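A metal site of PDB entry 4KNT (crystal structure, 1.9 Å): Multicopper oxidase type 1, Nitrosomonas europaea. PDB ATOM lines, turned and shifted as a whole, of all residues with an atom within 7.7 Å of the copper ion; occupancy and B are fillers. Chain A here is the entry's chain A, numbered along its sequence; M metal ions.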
ATOM      1  N   ALA A   9       2.365 -18.065 -17.535  1.00  0.00           N
ATOM      2  CA  ALA A   9       3.596 -18.837 -17.399  1.00  0.00           C
ATOM      3  C   ALA A   9       3.252 -20.315 -17.517  1.00  0.00           C
ATOM      4  O   ALA A   9       2.580 -20.874 -16.642  1.00  0.00           O
ATOM      5  CB  ALA A   9       4.272 -18.536 -16.073  1.00  0.00           C
ATOM      6  N   GLU A  11       4.637 -24.285 -18.496  1.00  0.00           N
ATOM      7  CA  GLU A  11       5.727 -25.236 -18.687  1.00  0.00           C
ATOM      8  C   GLU A  11       5.230 -26.381 -19.574  1.00  0.00           C
ATOM      9  O   GLU A  11       4.373 -27.166 -19.166  1.00  0.00           O
ATOM     10  CB  GLU A  11       6.223 -25.750 -17.332  1.00  0.00           C
ATOM     11  CG  GLU A  11       6.689 -24.638 -16.403  1.00  0.00           C
ATOM     12  CD  GLU A  11       6.988 -25.099 -14.972  1.00  0.00           C
ATOM     13  OE1 GLU A  11       6.892 -26.309 -14.691  1.00  0.00           O
ATOM     14  OE2 GLU A  11       7.311 -24.230 -14.133  1.00  0.00           O
ATOM     15  N   TRP A  26      10.035 -23.710 -20.591  1.00  0.00           N
ATOM     16  CA  TRP A  26       9.255 -22.825 -19.747  1.00  0.00           C
ATOM     17  C   TRP A  26       8.919 -21.625 -20.615  1.00  0.00           C
ATOM     18  O   TRP A  26       9.801 -21.063 -21.273  1.00  0.00           O
ATOM     19  CB  TRP A  26      10.056 -22.366 -18.526  1.00  0.00           C
ATOM     20  CG  TRP A  26      10.472 -23.455 -17.591  1.00  0.00           C
ATOM     21  CD1 TRP A  26      10.003 -24.745 -17.545  1.00  0.00           C
ATOM     22  CD2 TRP A  26      11.422 -23.352 -16.519  1.00  0.00           C
ATOM     23  NE1 TRP A  26      10.619 -25.441 -16.534  1.00  0.00           N
ATOM     24  CE2 TRP A  26      11.484 -24.608 -15.883  1.00  0.00           C
ATOM     25  CE3 TRP A  26      12.233 -22.306 -16.053  1.00  0.00           C
ATOM     26  CZ2 TRP A  26      12.333 -24.855 -14.800  1.00  0.00           C
ATOM     27  CZ3 TRP A  26      13.073 -22.555 -14.965  1.00  0.00           C
ATOM     28  CH2 TRP A  26      13.114 -23.815 -14.354  1.00  0.00           C
ATOM     29  N   THR A  27       7.649 -21.256 -20.647  1.00  0.00           N
ATOM     30  CA  THR A  27       7.167 -20.323 -21.667  1.00  0.00           C
ATOM     31  C   THR A  27       6.199 -19.283 -21.126  1.00  0.00           C
ATOM     32  O   THR A  27       5.655 -19.418 -20.030  1.00  0.00           O
ATOM     33  CB  THR A  27       6.435 -21.057 -22.817  1.00  0.00           C
ATOM     34  OG1 THR A  27       5.124 -21.440 -22.371  1.00  0.00           O
ATOM     35  CG2 THR A  27       7.190 -22.293 -23.288  1.00  0.00           C
ATOM     36  N   PHE A  28       5.986 -18.258 -21.937  1.00  0.00           N
ATOM     37  CA  PHE A  28       4.808 -17.419 -21.810  1.00  0.00           C
ATOM     38  C   PHE A  28       3.833 -17.862 -22.895  1.00  0.00           C
ATOM     39  O   PHE A  28       4.177 -17.900 -24.081  1.00  0.00           O
ATOM     40  CB  PHE A  28       5.163 -15.931 -21.957  1.00  0.00           C
ATOM     41  CG  PHE A  28       6.035 -15.397 -20.845  1.00  0.00           C
ATOM     42  CD1 PHE A  28       5.546 -15.270 -19.553  1.00  0.00           C
ATOM     43  CD2 PHE A  28       7.355 -15.023 -21.104  1.00  0.00           C
ATOM     44  CE1 PHE A  28       6.359 -14.782 -18.513  1.00  0.00           C
ATOM     45  CE2 PHE A  28       8.173 -14.541 -20.080  1.00  0.00           C
ATOM     46  CZ  PHE A  28       7.666 -14.417 -18.779  1.00  0.00           C
ATOM     47  N   LEU A  49       0.106 -11.375 -14.957  1.00  0.00           N
ATOM     48  CA  LEU A  49       0.780 -12.657 -15.113  1.00  0.00           C
ATOM     49  C   LEU A  49       0.033 -13.725 -14.325  1.00  0.00           C
ATOM     50  O   LEU A  49      -0.213 -13.562 -13.122  1.00  0.00           O
ATOM     51  CB  LEU A  49       2.238 -12.585 -14.645  1.00  0.00           C
ATOM     52  CG  LEU A  49       3.015 -13.910 -14.736  1.00  0.00           C
ATOM     53  CD1 LEU A  49       3.378 -14.230 -16.184  1.00  0.00           C
ATOM     54  CD2 LEU A  49       4.256 -13.884 -13.862  1.00  0.00           C
ATOM     55  N   ASN A  51       0.520 -17.615 -13.292  1.00  0.00           N
ATOM     56  CA  ASN A  51       1.364 -18.798 -13.280  1.00  0.00           C
ATOM     57  C   ASN A  51       0.475 -20.038 -13.309  1.00  0.00           C
ATOM     58  O   ASN A  51      -0.276 -20.287 -12.366  1.00  0.00           O
ATOM     59  CB  ASN A  51       2.307 -18.805 -12.071  1.00  0.00           C
ATOM     60  CG  ASN A  51       3.418 -19.859 -12.183  1.00  0.00           C
ATOM     61  OD1 ASN A  51       3.435 -20.668 -13.108  1.00  0.00           O
ATOM     62  ND2 ASN A  51       4.334 -19.853 -11.221  1.00  0.00           N
ATOM     63  N   ASN A  57       7.379 -24.550 -10.986  1.00  0.00           N
ATOM     64  CA  ASN A  57       8.290 -23.476 -10.608  1.00  0.00           C
ATOM     65  C   ASN A  57       7.583 -22.127 -10.476  1.00  0.00           C
ATOM     66  O   ASN A  57       6.576 -21.889 -11.129  1.00  0.00           O
ATOM     67  CB  ASN A  57       9.414 -23.333 -11.625  1.00  0.00           C
ATOM     68  CG  ASN A  57      10.178 -24.619 -11.827  1.00  0.00           C
ATOM     69  OD1 ASN A  57      11.123 -24.914 -11.089  1.00  0.00           O
ATOM     70  ND2 ASN A  57       9.780 -25.408 -12.826  1.00  0.00           N
ATOM     71  N   SER A  58       8.142 -21.267  -9.632  1.00  0.00           N
ATOM     72  CA  SER A  58       7.707 -19.872  -9.546  1.00  0.00           C
ATOM     73  C   SER A  58       8.235 -19.097 -10.753  1.00  0.00           C
ATOM     74  O   SER A  58       9.341 -19.340 -11.226  1.00  0.00           O
ATOM     75  CB  SER A  58       8.212 -19.240  -8.249  1.00  0.00           C
ATOM     76  OG  SER A  58       7.557 -19.813  -7.124  1.00  0.00           O
ATOM     77  N   HIS A  59       7.417 -18.159 -11.238  1.00  0.00           N
ATOM     78  CA  HIS A  59       7.773 -17.363 -12.400  1.00  0.00           C
ATOM     79  C   HIS A  59       7.434 -15.887 -12.170  1.00  0.00           C
ATOM     80  O   HIS A  59       6.759 -15.538 -11.201  1.00  0.00           O
ATOM     81  CB  HIS A  59       7.087 -17.889 -13.661  1.00  0.00           C
ATOM     82  CG  HIS A  59       7.458 -19.305 -13.995  1.00  0.00           C
ATOM     83  ND1 HIS A  59       8.720 -19.662 -14.436  1.00  0.00           N
ATOM     84  CD2 HIS A  59       6.741 -20.452 -13.950  1.00  0.00           C
ATOM     85  CE1 HIS A  59       8.751 -20.973 -14.644  1.00  0.00           C
ATOM     86  NE2 HIS A  59       7.566 -21.472 -14.357  1.00  0.00           N
ATOM     87  N   SER A  60       7.923 -15.023 -13.062  1.00  0.00           N
ATOM     88  CA  SER A  60       7.744 -13.590 -12.912  1.00  0.00           C
ATOM     89  C   SER A  60       7.805 -12.911 -14.275  1.00  0.00           C
ATOM     90  O   SER A  60       7.940 -13.582 -15.306  1.00  0.00           O
ATOM     91  CB  SER A  60       8.821 -13.014 -11.994  1.00  0.00           C
ATOM     92  OG  SER A  60      10.116 -13.280 -12.499  1.00  0.00           O
ATOM     93  N   MET A  61       7.694 -11.586 -14.287  1.00  0.00           N
ATOM     94  CA  MET A  61       7.852 -10.840 -15.534  1.00  0.00           C
ATOM     95  C   MET A  61       8.656  -9.555 -15.383  1.00  0.00           C
ATOM     96  O   MET A  61       8.389  -8.749 -14.494  1.00  0.00           O
ATOM     97  CB  MET A  61       6.493 -10.540 -16.179  1.00  0.00           C
ATOM     98  CG  MET A  61       6.585  -9.631 -17.388  1.00  0.00           C
ATOM     99  SD  MET A  61       7.435 -10.370 -18.803  1.00  0.00           S
ATOM    100  CE  MET A  61       6.072 -11.257 -19.539  1.00  0.00           C
ATOM    101  N   SER A  76       8.720 -13.027  -7.979  1.00  0.00           N
ATOM    102  CA  SER A  76       8.292 -14.356  -8.397  1.00  0.00           C
ATOM    103  C   SER A  76       6.978 -14.772  -7.751  1.00  0.00           C
ATOM    104  O   SER A  76       6.737 -14.509  -6.572  1.00  0.00           O
ATOM    105  CB  SER A  76       9.365 -15.404  -8.076  1.00  0.00           C
ATOM    106  OG  SER A  76      10.573 -15.109  -8.756  1.00  0.00           O
ATOM    107  N   HIS A  98      11.333 -10.748 -20.255  1.00  0.00           N
ATOM    108  CA  HIS A  98      11.673 -12.106 -19.805  1.00  0.00           C
ATOM    109  C   HIS A  98      11.246 -12.355 -18.372  1.00  0.00           C
ATOM    110  O   HIS A  98      10.963 -11.406 -17.635  1.00  0.00           O
ATOM    111  CB  HIS A  98      13.174 -12.354 -19.951  1.00  0.00           C
ATOM    112  CG  HIS A  98      14.031 -11.399 -19.175  1.00  0.00           C
ATOM    113  ND1 HIS A  98      14.389 -11.608 -17.860  1.00  0.00           N
ATOM    114  CD2 HIS A  98      14.597 -10.217 -19.536  1.00  0.00           C
ATOM    115  CE1 HIS A  98      15.132 -10.606 -17.439  1.00  0.00           C
ATOM    116  NE2 HIS A  98      15.284  -9.750 -18.439  1.00  0.00           N
ATOM    117  N   CYS A  99      11.181 -13.621 -17.995  1.00  0.00           N
ATOM    118  CA  CYS A  99      10.994 -14.003 -16.600  1.00  0.00           C
ATOM    119  C   CYS A  99      12.219 -13.575 -15.803  1.00  0.00           C
ATOM    120  O   CYS A  99      13.350 -13.693 -16.270  1.00  0.00           O
ATOM    121  CB  CYS A  99      10.772 -15.516 -16.489  1.00  0.00           C
ATOM    122  SG  CYS A  99      10.529 -16.113 -14.810  1.00  0.00           S
ATOM    123  N   GLY A 100      11.975 -13.048 -14.604  1.00  0.00           N
ATOM    124  CA  GLY A 100      13.053 -12.595 -13.728  1.00  0.00           C
ATOM    125  C   GLY A 100      13.251 -13.482 -12.510  1.00  0.00           C
ATOM    126  O   GLY A 100      13.835 -13.047 -11.506  1.00  0.00           O
ATOM    127  N   SER A 101      12.793 -14.726 -12.595  1.00  0.00           N
ATOM    128  CA  SER A 101      12.860 -15.659 -11.459  1.00  0.00           C
ATOM    129  C   SER A 101      14.209 -16.361 -11.331  1.00  0.00           C
ATOM    130  O   SER A 101      15.019 -16.342 -12.256  1.00  0.00           O
ATOM    131  CB  SER A 101      11.724 -16.672 -11.528  1.00  0.00           C
ATOM    132  OG  SER A 101      10.474 -16.011 -11.407  1.00  0.00           O
ATOM    133  N   ASP A 102      14.420 -16.990 -10.182  1.00  0.00           N
ATOM    134  CA  ASP A 102      15.716 -17.555  -9.799  1.00  0.00           C
ATOM    135  C   ASP A 102      15.903 -18.997 -10.299  1.00  0.00           C
ATOM    136  O   ASP A 102      15.070 -19.862 -10.014  1.00  0.00           O
ATOM    137  CB  ASP A 102      15.855 -17.480  -8.272  1.00  0.00           C
ATOM    138  CG  ASP A 102      17.188 -18.022  -7.776  1.00  0.00           C
ATOM    139  OD1 ASP A 102      18.235 -17.681  -8.352  1.00  0.00           O
ATOM    140  OD2 ASP A 102      17.171 -18.786  -6.787  1.00  0.00           O
ATOM    141  N   PRO A 103      16.977 -19.256 -11.069  1.00  0.00           N
ATOM    142  CA  PRO A 103      17.954 -18.300 -11.588  1.00  0.00           C
ATOM    143  C   PRO A 103      17.572 -17.799 -12.991  1.00  0.00           C
ATOM    144  O   PRO A 103      17.198 -18.595 -13.843  1.00  0.00           O
ATOM    145  CB  PRO A 103      19.241 -19.114 -11.637  1.00  0.00           C
ATOM    146  CG  PRO A 103      18.794 -20.537 -11.863  1.00  0.00           C
ATOM    147  CD  PRO A 103      17.359 -20.652 -11.393  1.00  0.00           C
ATOM    148  N   MET A 104      17.686 -16.498 -13.223  1.00  0.00           N
ATOM    149  CA  MET A 104      17.288 -15.915 -14.507  1.00  0.00           C
ATOM    150  C   MET A 104      17.920 -16.601 -15.698  1.00  0.00           C
ATOM    151  O   MET A 104      17.285 -16.769 -16.737  1.00  0.00           O
ATOM    152  CB  MET A 104      17.577 -14.417 -14.551  1.00  0.00           C
ATOM    153  CG  MET A 104      16.521 -13.576 -13.866  1.00  0.00           C
ATOM    154  SD  MET A 104      16.750 -11.817 -14.160  1.00  0.00           S
ATOM    155  CE  MET A 104      18.006 -11.417 -12.940  1.00  0.00           C
ATOM    156  N   GLN A 106      18.486 -19.671 -16.279  1.00  0.00           N
ATOM    157  CA  GLN A 106      17.710 -20.849 -16.669  1.00  0.00           C
ATOM    158  C   GLN A 106      16.314 -20.497 -17.203  1.00  0.00           C
ATOM    159  O   GLN A 106      15.862 -21.083 -18.195  1.00  0.00           O
ATOM    160  CB  GLN A 106      17.599 -21.830 -15.503  1.00  0.00           C
ATOM    161  CG  GLN A 106      16.982 -23.177 -15.853  1.00  0.00           C
ATOM    162  CD  GLN A 106      16.776 -24.052 -14.637  1.00  0.00           C
ATOM    163  OE1 GLN A 106      16.571 -23.550 -13.532  1.00  0.00           O
ATOM    164  NE2 GLN A 106      16.812 -25.365 -14.836  1.00  0.00           N
ATOM    165  N   HIS A 107      15.631 -19.568 -16.545  1.00  0.00           N
ATOM    166  CA  HIS A 107      14.298 -19.168 -16.973  1.00  0.00           C
ATOM    167  C   HIS A 107      14.319 -18.581 -18.385  1.00  0.00           C
ATOM    168  O   HIS A 107      13.463 -18.910 -19.215  1.00  0.00           O
ATOM    169  CB  HIS A 107      13.645 -18.215 -15.970  1.00  0.00           C
ATOM    170  CG  HIS A 107      13.271 -18.871 -14.674  1.00  0.00           C
ATOM    171  ND1 HIS A 107      11.993 -19.282 -14.387  1.00  0.00           N
ATOM    172  CD2 HIS A 107      14.030 -19.203 -13.600  1.00  0.00           C
ATOM    173  CE1 HIS A 107      11.970 -19.824 -13.181  1.00  0.00           C
ATOM    174  NE2 HIS A 107      13.193 -19.791 -12.685  1.00  0.00           N
ATOM    175  N   ILE A 108      15.324 -17.749 -18.672  1.00  0.00           N
ATOM    176  CA  ILE A 108      15.531 -17.242 -20.025  1.00  0.00           C
ATOM    177  C   ILE A 108      15.874 -18.384 -20.999  1.00  0.00           C
ATOM    178  O   ILE A 108      15.229 -18.534 -22.029  1.00  0.00           O
ATOM    179  CB  ILE A 108      16.616 -16.126 -20.078  1.00  0.00           C
ATOM    180  CG1 ILE A 108      16.149 -14.882 -19.315  1.00  0.00           C
ATOM    181  CG2 ILE A 108      16.944 -15.751 -21.534  1.00  0.00           C
ATOM    182  CD1 ILE A 108      17.230 -13.817 -19.104  1.00  0.00           C
ATOM    183  N   ARG A 110      15.339 -21.524 -20.945  1.00  0.00           N
ATOM    184  CA  ARG A 110      14.268 -22.501 -21.174  1.00  0.00           C
ATOM    185  C   ARG A 110      13.113 -21.943 -22.006  1.00  0.00           C
ATOM    186  O   ARG A 110      12.215 -22.691 -22.403  1.00  0.00           O
ATOM    187  CB  ARG A 110      13.794 -23.124 -19.865  1.00  0.00           C
ATOM    188  CG  ARG A 110      14.875 -23.959 -19.177  1.00  0.00           C
ATOM    189  CD  ARG A 110      14.355 -24.703 -17.966  1.00  0.00           C
ATOM    190  NE  ARG A 110      13.532 -25.845 -18.348  1.00  0.00           N
ATOM    191  CZ  ARG A 110      13.417 -26.964 -17.635  1.00  0.00           C
ATOM    192  NH1 ARG A 110      14.085 -27.101 -16.492  1.00  0.00           N
ATOM    193  NH2 ARG A 110      12.646 -27.946 -18.061  1.00  0.00           N
ATOM    194  N   MET A 112      11.541 -18.426 -21.581  1.00  0.00           N
ATOM    195  CA  MET A 112      10.693 -17.350 -21.034  1.00  0.00           C
ATOM    196  C   MET A 112      11.193 -15.982 -21.444  1.00  0.00           C
ATOM    197  O   MET A 112      11.727 -15.222 -20.622  1.00  0.00           O
ATOM    198  CB  MET A 112      10.563 -17.464 -19.511  1.00  0.00           C
ATOM    199  CG  MET A 112      10.060 -18.815 -19.050  1.00  0.00           C
ATOM    200  SD  MET A 112       9.463 -18.873 -17.360  1.00  0.00           S
ATOM    201  CE  MET A 112       7.877 -18.043 -17.546  1.00  0.00           C
HETATM  202 CU    CU M   1      10.230 -18.299 -15.099  1.00  0.00          CU
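The side-chain sulfur of Cys 99 lies close to the side-chain hydroxyl of Ser 101 (3.4 Å).
The side-chain sulfur (SG) of Cys 99 lies close to the backbone NH (N) of Ser 60 (3.3 Å).
O of Asp 102 sits at hydrogen-bond distance from NE2 of His 107 (3.3 Å).
O of Trp 26 lies close to N of Met 112 (3.2 Å).
A ring nitrogen (NE2) of His 59 sits close to the backbone carbonyl oxygen (O) of Asn 57.
NE2 of His 59 sits at hydrogen-bond distance from OE2 of Glu 11 (2.8 Å).
The copper ion is bound by a ring nitrogen (ND1) of His 59, at 2.1 Å.
ND1 of His 107 binds the copper ion, at 2.1 Å.
The copper ion is bound by SG of Cys 99.
The copper ion is bound by SD of Met 112.
The copper ion has four donor atoms within binding distance.
Four residues have an atom within 4 Å of the copper ion: His 59, Cys 99, His 107 and Met 112.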
